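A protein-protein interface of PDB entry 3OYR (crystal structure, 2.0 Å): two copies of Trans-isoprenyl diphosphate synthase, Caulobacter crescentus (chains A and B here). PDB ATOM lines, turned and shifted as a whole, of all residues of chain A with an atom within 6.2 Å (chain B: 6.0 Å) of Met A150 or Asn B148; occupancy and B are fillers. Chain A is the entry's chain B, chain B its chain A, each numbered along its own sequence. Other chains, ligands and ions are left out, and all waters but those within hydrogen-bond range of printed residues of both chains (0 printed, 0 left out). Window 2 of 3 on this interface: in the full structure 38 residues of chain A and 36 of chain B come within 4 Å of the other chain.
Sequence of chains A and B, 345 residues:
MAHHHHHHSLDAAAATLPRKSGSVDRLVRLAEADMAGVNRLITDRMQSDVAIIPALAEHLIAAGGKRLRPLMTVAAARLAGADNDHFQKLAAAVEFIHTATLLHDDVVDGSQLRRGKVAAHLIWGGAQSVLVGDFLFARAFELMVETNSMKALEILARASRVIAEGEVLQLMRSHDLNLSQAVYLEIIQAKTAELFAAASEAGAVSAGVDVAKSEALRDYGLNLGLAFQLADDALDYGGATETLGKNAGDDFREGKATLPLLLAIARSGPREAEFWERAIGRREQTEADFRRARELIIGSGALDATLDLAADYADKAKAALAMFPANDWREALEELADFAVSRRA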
ATOM      1  N   THR A 147      19.568   3.862  -1.787  1.00  0.00           N
ATOM      2  CA  THR A 147      18.948   3.358  -3.016  1.00  0.00           C
ATOM      3  C   THR A 147      19.116   4.326  -4.188  1.00  0.00           C
ATOM      4  O   THR A 147      18.934   3.926  -5.348  1.00  0.00           O
ATOM      5  CB  THR A 147      17.437   3.112  -2.844  1.00  0.00           C
ATOM      6  OG1 THR A 147      16.745   4.363  -2.911  1.00  0.00           O
ATOM      7  CG2 THR A 147      17.142   2.458  -1.509  1.00  0.00           C
ATOM      8  N   ASN A 148      19.411   5.599  -3.883  1.00  0.00           N
ATOM      9  CA  ASN A 148      19.554   6.653  -4.907  1.00  0.00           C
ATOM     10  C   ASN A 148      18.267   6.945  -5.687  1.00  0.00           C
ATOM     11  O   ASN A 148      18.296   7.494  -6.780  1.00  0.00           O
ATOM     12  CB  ASN A 148      20.697   6.325  -5.884  1.00  0.00           C
ATOM     13  CG  ASN A 148      21.795   7.338  -5.849  1.00  0.00           C
ATOM     14  OD1 ASN A 148      21.584   8.513  -5.517  1.00  0.00           O
ATOM     15  ND2 ASN A 148      22.988   6.900  -6.204  1.00  0.00           N
ATOM     16  N   SER A 149      17.129   6.566  -5.133  1.00  0.00           N
ATOM     17  CA  SER A 149      15.880   6.867  -5.791  1.00  0.00           C
ATOM     18  C   SER A 149      15.253   8.084  -5.161  1.00  0.00           C
ATOM     19  O   SER A 149      14.651   8.027  -4.072  1.00  0.00           O
ATOM     20  CB  SER A 149      14.922   5.682  -5.783  1.00  0.00           C
ATOM     21  OG  SER A 149      13.692   6.103  -6.355  1.00  0.00           O
ATOM     22  N   MET A 150      15.426   9.201  -5.849  1.00  0.00           N
ATOM     23  CA  MET A 150      14.906  10.465  -5.350  1.00  0.00           C
ATOM     24  C   MET A 150      13.381  10.487  -5.299  1.00  0.00           C
ATOM     25  O   MET A 150      12.781  11.060  -4.379  1.00  0.00           O
ATOM     26  CB  MET A 150      15.495  11.659  -6.121  1.00  0.00           C
ATOM     27  CG  MET A 150      15.128  13.014  -5.510  1.00  0.00           C
ATOM     28  SD  MET A 150      15.832  13.479  -3.894  1.00  0.00           S
ATOM     29  CE  MET A 150      16.181  12.015  -3.002  1.00  0.00           C
ATOM     30  N   LYS A 151      12.761   9.812  -6.262  1.00  0.00           N
ATOM     31  CA  LYS A 151      11.307   9.697  -6.293  1.00  0.00           C
ATOM     32  C   LYS A 151      10.810   8.869  -5.106  1.00  0.00           C
ATOM     33  O   LYS A 151       9.865   9.272  -4.414  1.00  0.00           O
ATOM     34  CB  LYS A 151      10.838   9.122  -7.650  1.00  0.00           C
ATOM     35  CG  LYS A 151       9.322   8.991  -7.800  1.00  0.00           C
ATOM     36  CD  LYS A 151       8.591  10.335  -7.877  1.00  0.00           C
ATOM     37  CE  LYS A 151       7.101  10.112  -8.171  1.00  0.00           C
ATOM     38  NZ  LYS A 151       6.352  11.359  -8.509  1.00  0.00           N
ATOM     39  N   ALA A 152      11.474   7.750  -4.808  1.00  0.00           N
ATOM     40  CA  ALA A 152      11.008   6.943  -3.687  1.00  0.00           C
ATOM     41  C   ALA A 152      11.187   7.708  -2.384  1.00  0.00           C
ATOM     42  O   ALA A 152      10.366   7.604  -1.476  1.00  0.00           O
ATOM     43  CB  ALA A 152      11.727   5.601  -3.641  1.00  0.00           C
ATOM     44  N   LEU A 153      12.262   8.484  -2.294  1.00  0.00           N
ATOM     45  CA  LEU A 153      12.486   9.320  -1.118  1.00  0.00           C
ATOM     46  C   LEU A 153      11.435  10.427  -0.939  1.00  0.00           C
ATOM     47  O   LEU A 153      10.979  10.684   0.167  1.00  0.00           O
ATOM     48  CB  LEU A 153      13.891   9.911  -1.146  1.00  0.00           C
ATOM     49  CG  LEU A 153      14.504  10.031   0.246  1.00  0.00           C
ATOM     50  CD1 LEU A 153      15.991   9.819   0.178  1.00  0.00           C
ATOM     51  CD2 LEU A 153      14.207  11.390   0.855  1.00  0.00           C
ATOM     52  N   GLU A 154      11.032  11.066  -2.025  1.00  0.00           N
ATOM     53  CA  GLU A 154       9.957  12.080  -1.970  1.00  0.00           C
ATOM     54  C   GLU A 154       8.633  11.461  -1.520  1.00  0.00           C
ATOM     55  O   GLU A 154       7.899  12.051  -0.721  1.00  0.00           O
ATOM     56  CB  GLU A 154       9.802  12.746  -3.343  1.00  0.00           C
ATOM     57  CG  GLU A 154       8.490  13.470  -3.605  1.00  0.00           C
ATOM     58  CD  GLU A 154       8.158  13.409  -5.073  1.00  0.00           C
ATOM     59  OE1 GLU A 154       7.273  12.609  -5.453  1.00  0.00           O
ATOM     60  OE2 GLU A 154       8.825  14.120  -5.858  1.00  0.00           O
ATOM     61  N   ILE A 155       8.364  10.256  -2.012  1.00  0.00           N
ATOM     62  CA  ILE A 155       7.142   9.547  -1.692  1.00  0.00           C
ATOM     63  C   ILE A 155       7.064   9.263  -0.194  1.00  0.00           C
ATOM     64  O   ILE A 155       6.037   9.497   0.426  1.00  0.00           O
ATOM     65  CB  ILE A 155       7.033   8.225  -2.494  1.00  0.00           C
ATOM     66  CG1 ILE A 155       6.678   8.489  -3.968  1.00  0.00           C
ATOM     67  CG2 ILE A 155       5.972   7.317  -1.920  1.00  0.00           C
ATOM     68  CD1 ILE A 155       6.884   7.202  -4.837  1.00  0.00           C
ATOM     69  N   HIS B  86      19.761  26.728  -4.385  1.00  0.00           N
ATOM     70  CA  HIS B  86      19.358  25.522  -3.653  1.00  0.00           C
ATOM     71  C   HIS B  86      19.629  25.572  -2.167  1.00  0.00           C
ATOM     72  O   HIS B  86      18.876  24.992  -1.394  1.00  0.00           O
ATOM     73  CB  HIS B  86      20.011  24.272  -4.246  1.00  0.00           C
ATOM     74  CG  HIS B  86      19.434  23.851  -5.562  1.00  0.00           C
ATOM     75  ND1 HIS B  86      20.169  23.176  -6.514  1.00  0.00           N
ATOM     76  CD2 HIS B  86      18.193  24.007  -6.085  1.00  0.00           C
ATOM     77  CE1 HIS B  86      19.406  22.932  -7.566  1.00  0.00           C
ATOM     78  NE2 HIS B  86      18.204  23.428  -7.333  1.00  0.00           N
ATOM     79  N   MET B 144      14.305  19.295   1.264  1.00  0.00           N
ATOM     80  CA  MET B 144      15.548  18.842   0.684  1.00  0.00           C
ATOM     81  C   MET B 144      15.404  18.083  -0.640  1.00  0.00           C
ATOM     82  O   MET B 144      16.258  18.222  -1.513  1.00  0.00           O
ATOM     83  CB  MET B 144      16.306  18.020   1.692  1.00  0.00           C
ATOM     84  CG  MET B 144      16.769  18.876   2.820  1.00  0.00           C
ATOM     85  SD  MET B 144      18.010  18.137   3.835  1.00  0.00           S
ATOM     86  CE  MET B 144      17.275  16.543   4.263  1.00  0.00           C
ATOM     87  N   VAL B 145      14.334  17.291  -0.774  1.00  0.00           N
ATOM     88  CA  VAL B 145      13.982  16.614  -2.032  1.00  0.00           C
ATOM     89  C   VAL B 145      13.790  17.619  -3.163  1.00  0.00           C
ATOM     90  O   VAL B 145      14.223  17.388  -4.301  1.00  0.00           O
ATOM     91  CB  VAL B 145      12.703  15.727  -1.866  1.00  0.00           C
ATOM     92  CG1 VAL B 145      12.062  15.387  -3.215  1.00  0.00           C
ATOM     93  CG2 VAL B 145      13.016  14.461  -1.086  1.00  0.00           C
ATOM     94  N   GLU B 146      13.176  18.752  -2.849  1.00  0.00           N
ATOM     95  CA  GLU B 146      13.012  19.833  -3.835  1.00  0.00           C
ATOM     96  C   GLU B 146      14.317  20.339  -4.455  1.00  0.00           C
ATOM     97  O   GLU B 146      14.284  20.875  -5.552  1.00  0.00           O
ATOM     98  CB  GLU B 146      12.302  21.044  -3.232  1.00  0.00           C
ATOM     99  CG  GLU B 146      10.843  20.864  -2.808  1.00  0.00           C
ATOM    100  CD  GLU B 146      10.251  22.177  -2.306  1.00  0.00           C
ATOM    101  OE1 GLU B 146       9.504  22.168  -1.301  1.00  0.00           O
ATOM    102  OE2 GLU B 146      10.560  23.236  -2.909  1.00  0.00           O
ATOM    103  N   THR B 147      15.448  20.198  -3.759  1.00  0.00           N
ATOM    104  CA  THR B 147      16.727  20.689  -4.299  1.00  0.00           C
ATOM    105  C   THR B 147      17.342  19.701  -5.283  1.00  0.00           C
ATOM    106  O   THR B 147      18.310  20.039  -5.981  1.00  0.00           O
ATOM    107  CB  THR B 147      17.778  20.965  -3.200  1.00  0.00           C
ATOM    108  OG1 THR B 147      18.182  19.732  -2.574  1.00  0.00           O
ATOM    109  CG2 THR B 147      17.238  21.934  -2.161  1.00  0.00           C
ATOM    110  N   ASN B 148      16.796  18.477  -5.300  1.00  0.00           N
ATOM    111  CA  ASN B 148      17.369  17.336  -6.021  1.00  0.00           C
ATOM    112  C   ASN B 148      18.810  17.006  -5.657  1.00  0.00           C
ATOM    113  O   ASN B 148      19.510  16.390  -6.459  1.00  0.00           O
ATOM    114  CB  ASN B 148      17.280  17.529  -7.541  1.00  0.00           C
ATOM    115  CG  ASN B 148      16.042  16.920  -8.128  1.00  0.00           C
ATOM    116  OD1 ASN B 148      15.846  15.698  -8.075  1.00  0.00           O
ATOM    117  ND2 ASN B 148      15.186  17.766  -8.702  1.00  0.00           N
ATOM    118  N   SER B 149      19.260  17.433  -4.475  1.00  0.00           N
ATOM    119  CA  SER B 149      20.637  17.179  -4.076  1.00  0.00           C
ATOM    120  C   SER B 149      20.727  15.958  -3.158  1.00  0.00           C
ATOM    121  O   SER B 149      20.472  16.048  -1.954  1.00  0.00           O
ATOM    122  CB  SER B 149      21.256  18.415  -3.420  1.00  0.00           C
ATOM    123  OG  SER B 149      22.575  18.094  -2.988  1.00  0.00           O
ATOM    124  N   MET B 150      21.074  14.814  -3.735  1.00  0.00           N
ATOM    125  CA  MET B 150      21.150  13.578  -2.959  1.00  0.00           C
ATOM    126  C   MET B 150      22.263  13.607  -1.911  1.00  0.00           C
ATOM    127  O   MET B 150      22.107  13.067  -0.814  1.00  0.00           O
ATOM    128  CB  MET B 150      21.250  12.335  -3.854  1.00  0.00           C
ATOM    129  CG  MET B 150      21.099  11.017  -3.077  1.00  0.00           C
ATOM    130  SD  MET B 150      19.397  10.622  -2.609  1.00  0.00           S
ATOM    131  CE  MET B 150      19.223  11.193  -1.015  1.00  0.00           C
ATOM    132  N   LEU B 153      20.924  15.548   1.137  1.00  0.00           N
ATOM    133  CA  LEU B 153      20.007  14.710   1.903  1.00  0.00           C
ATOM    134  C   LEU B 153      20.771  13.684   2.737  1.00  0.00           C
ATOM    135  O   LEU B 153      20.425  13.417   3.887  1.00  0.00           O
ATOM    136  CB  LEU B 153      19.021  14.002   0.972  1.00  0.00           C
ATOM    137  CG  LEU B 153      17.739  14.764   0.635  1.00  0.00           C
ATOM    138  CD1 LEU B 153      17.521  14.815  -0.870  1.00  0.00           C
ATOM    139  CD2 LEU B 153      16.541  14.138   1.334  1.00  0.00           C
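The side-chain carboxylate (OE1) of Glu A154 is in salt-bridge range of the side-chain amino group (NZ) of Lys A151, at 3.4 Å.
Asn A148 touches Met B150 (OD1 to CG, 3.5 Å).
Met A150 touches Asn B148 (CG to OD1, 3.8 Å).
Met A150 touches Met B150 (CE to SD, 3.5 Å).
Leu B153 touches Met A150 (CD1 to SD, 3.7 Å).
Leu A153 touches Val B145 (CD2 to CG2, 3.8 Å).
CD1 of Leu A153 touches CE of Met B150 (3.7 Å).
Leu A153 touches Leu B153.
Glu A154 touches Val B145.
Asn B148 touches one residue of chain A.
Of the printed residues of chain A, Met B150 touches Asn A148, Met A150 and Leu A153.
Of the printed residues of chain A, Val B145 touches Leu A153 (3.8 Å) and Glu A154 (3.5 Å).
Of the printed residues of chain A, Leu B153 touches Met A150 and Leu A153.
Printed residues of chain B within 4 Å of Glu A154: Val B145.
Ala A152 touches none of the printed residues of chain B.
The nearest residue of chain B that does not touch Met A150 is Val B145 (4.1 Å).
The nearest printed residue of chain A that does not touch Asn B148 is Lys A151 (6.9 Å).
Hydrophobic or aromatic side chains of chain B within 4 Å of the printed part of chain A: Val B145, Met B150 and Leu B153.
Among the printed residues, 8 pairs touch across the chains.
Asn A148 touches Met B150, and with the chains exchanged Met A150 touches Asn B148.
Met B150 touches its own counterpart, Met A150.
Met A150 touches Leu B153, and with the chains exchanged Leu A153 touches Met B150.
Leu B153 touches its own counterpart, Leu A153.
Positions printed for both chains: 147, 148, 149, 150 and 153.
Of the 8 pairs that touch across the chains among the printed residues, 6 have their exchanged pair printed and touching as well.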
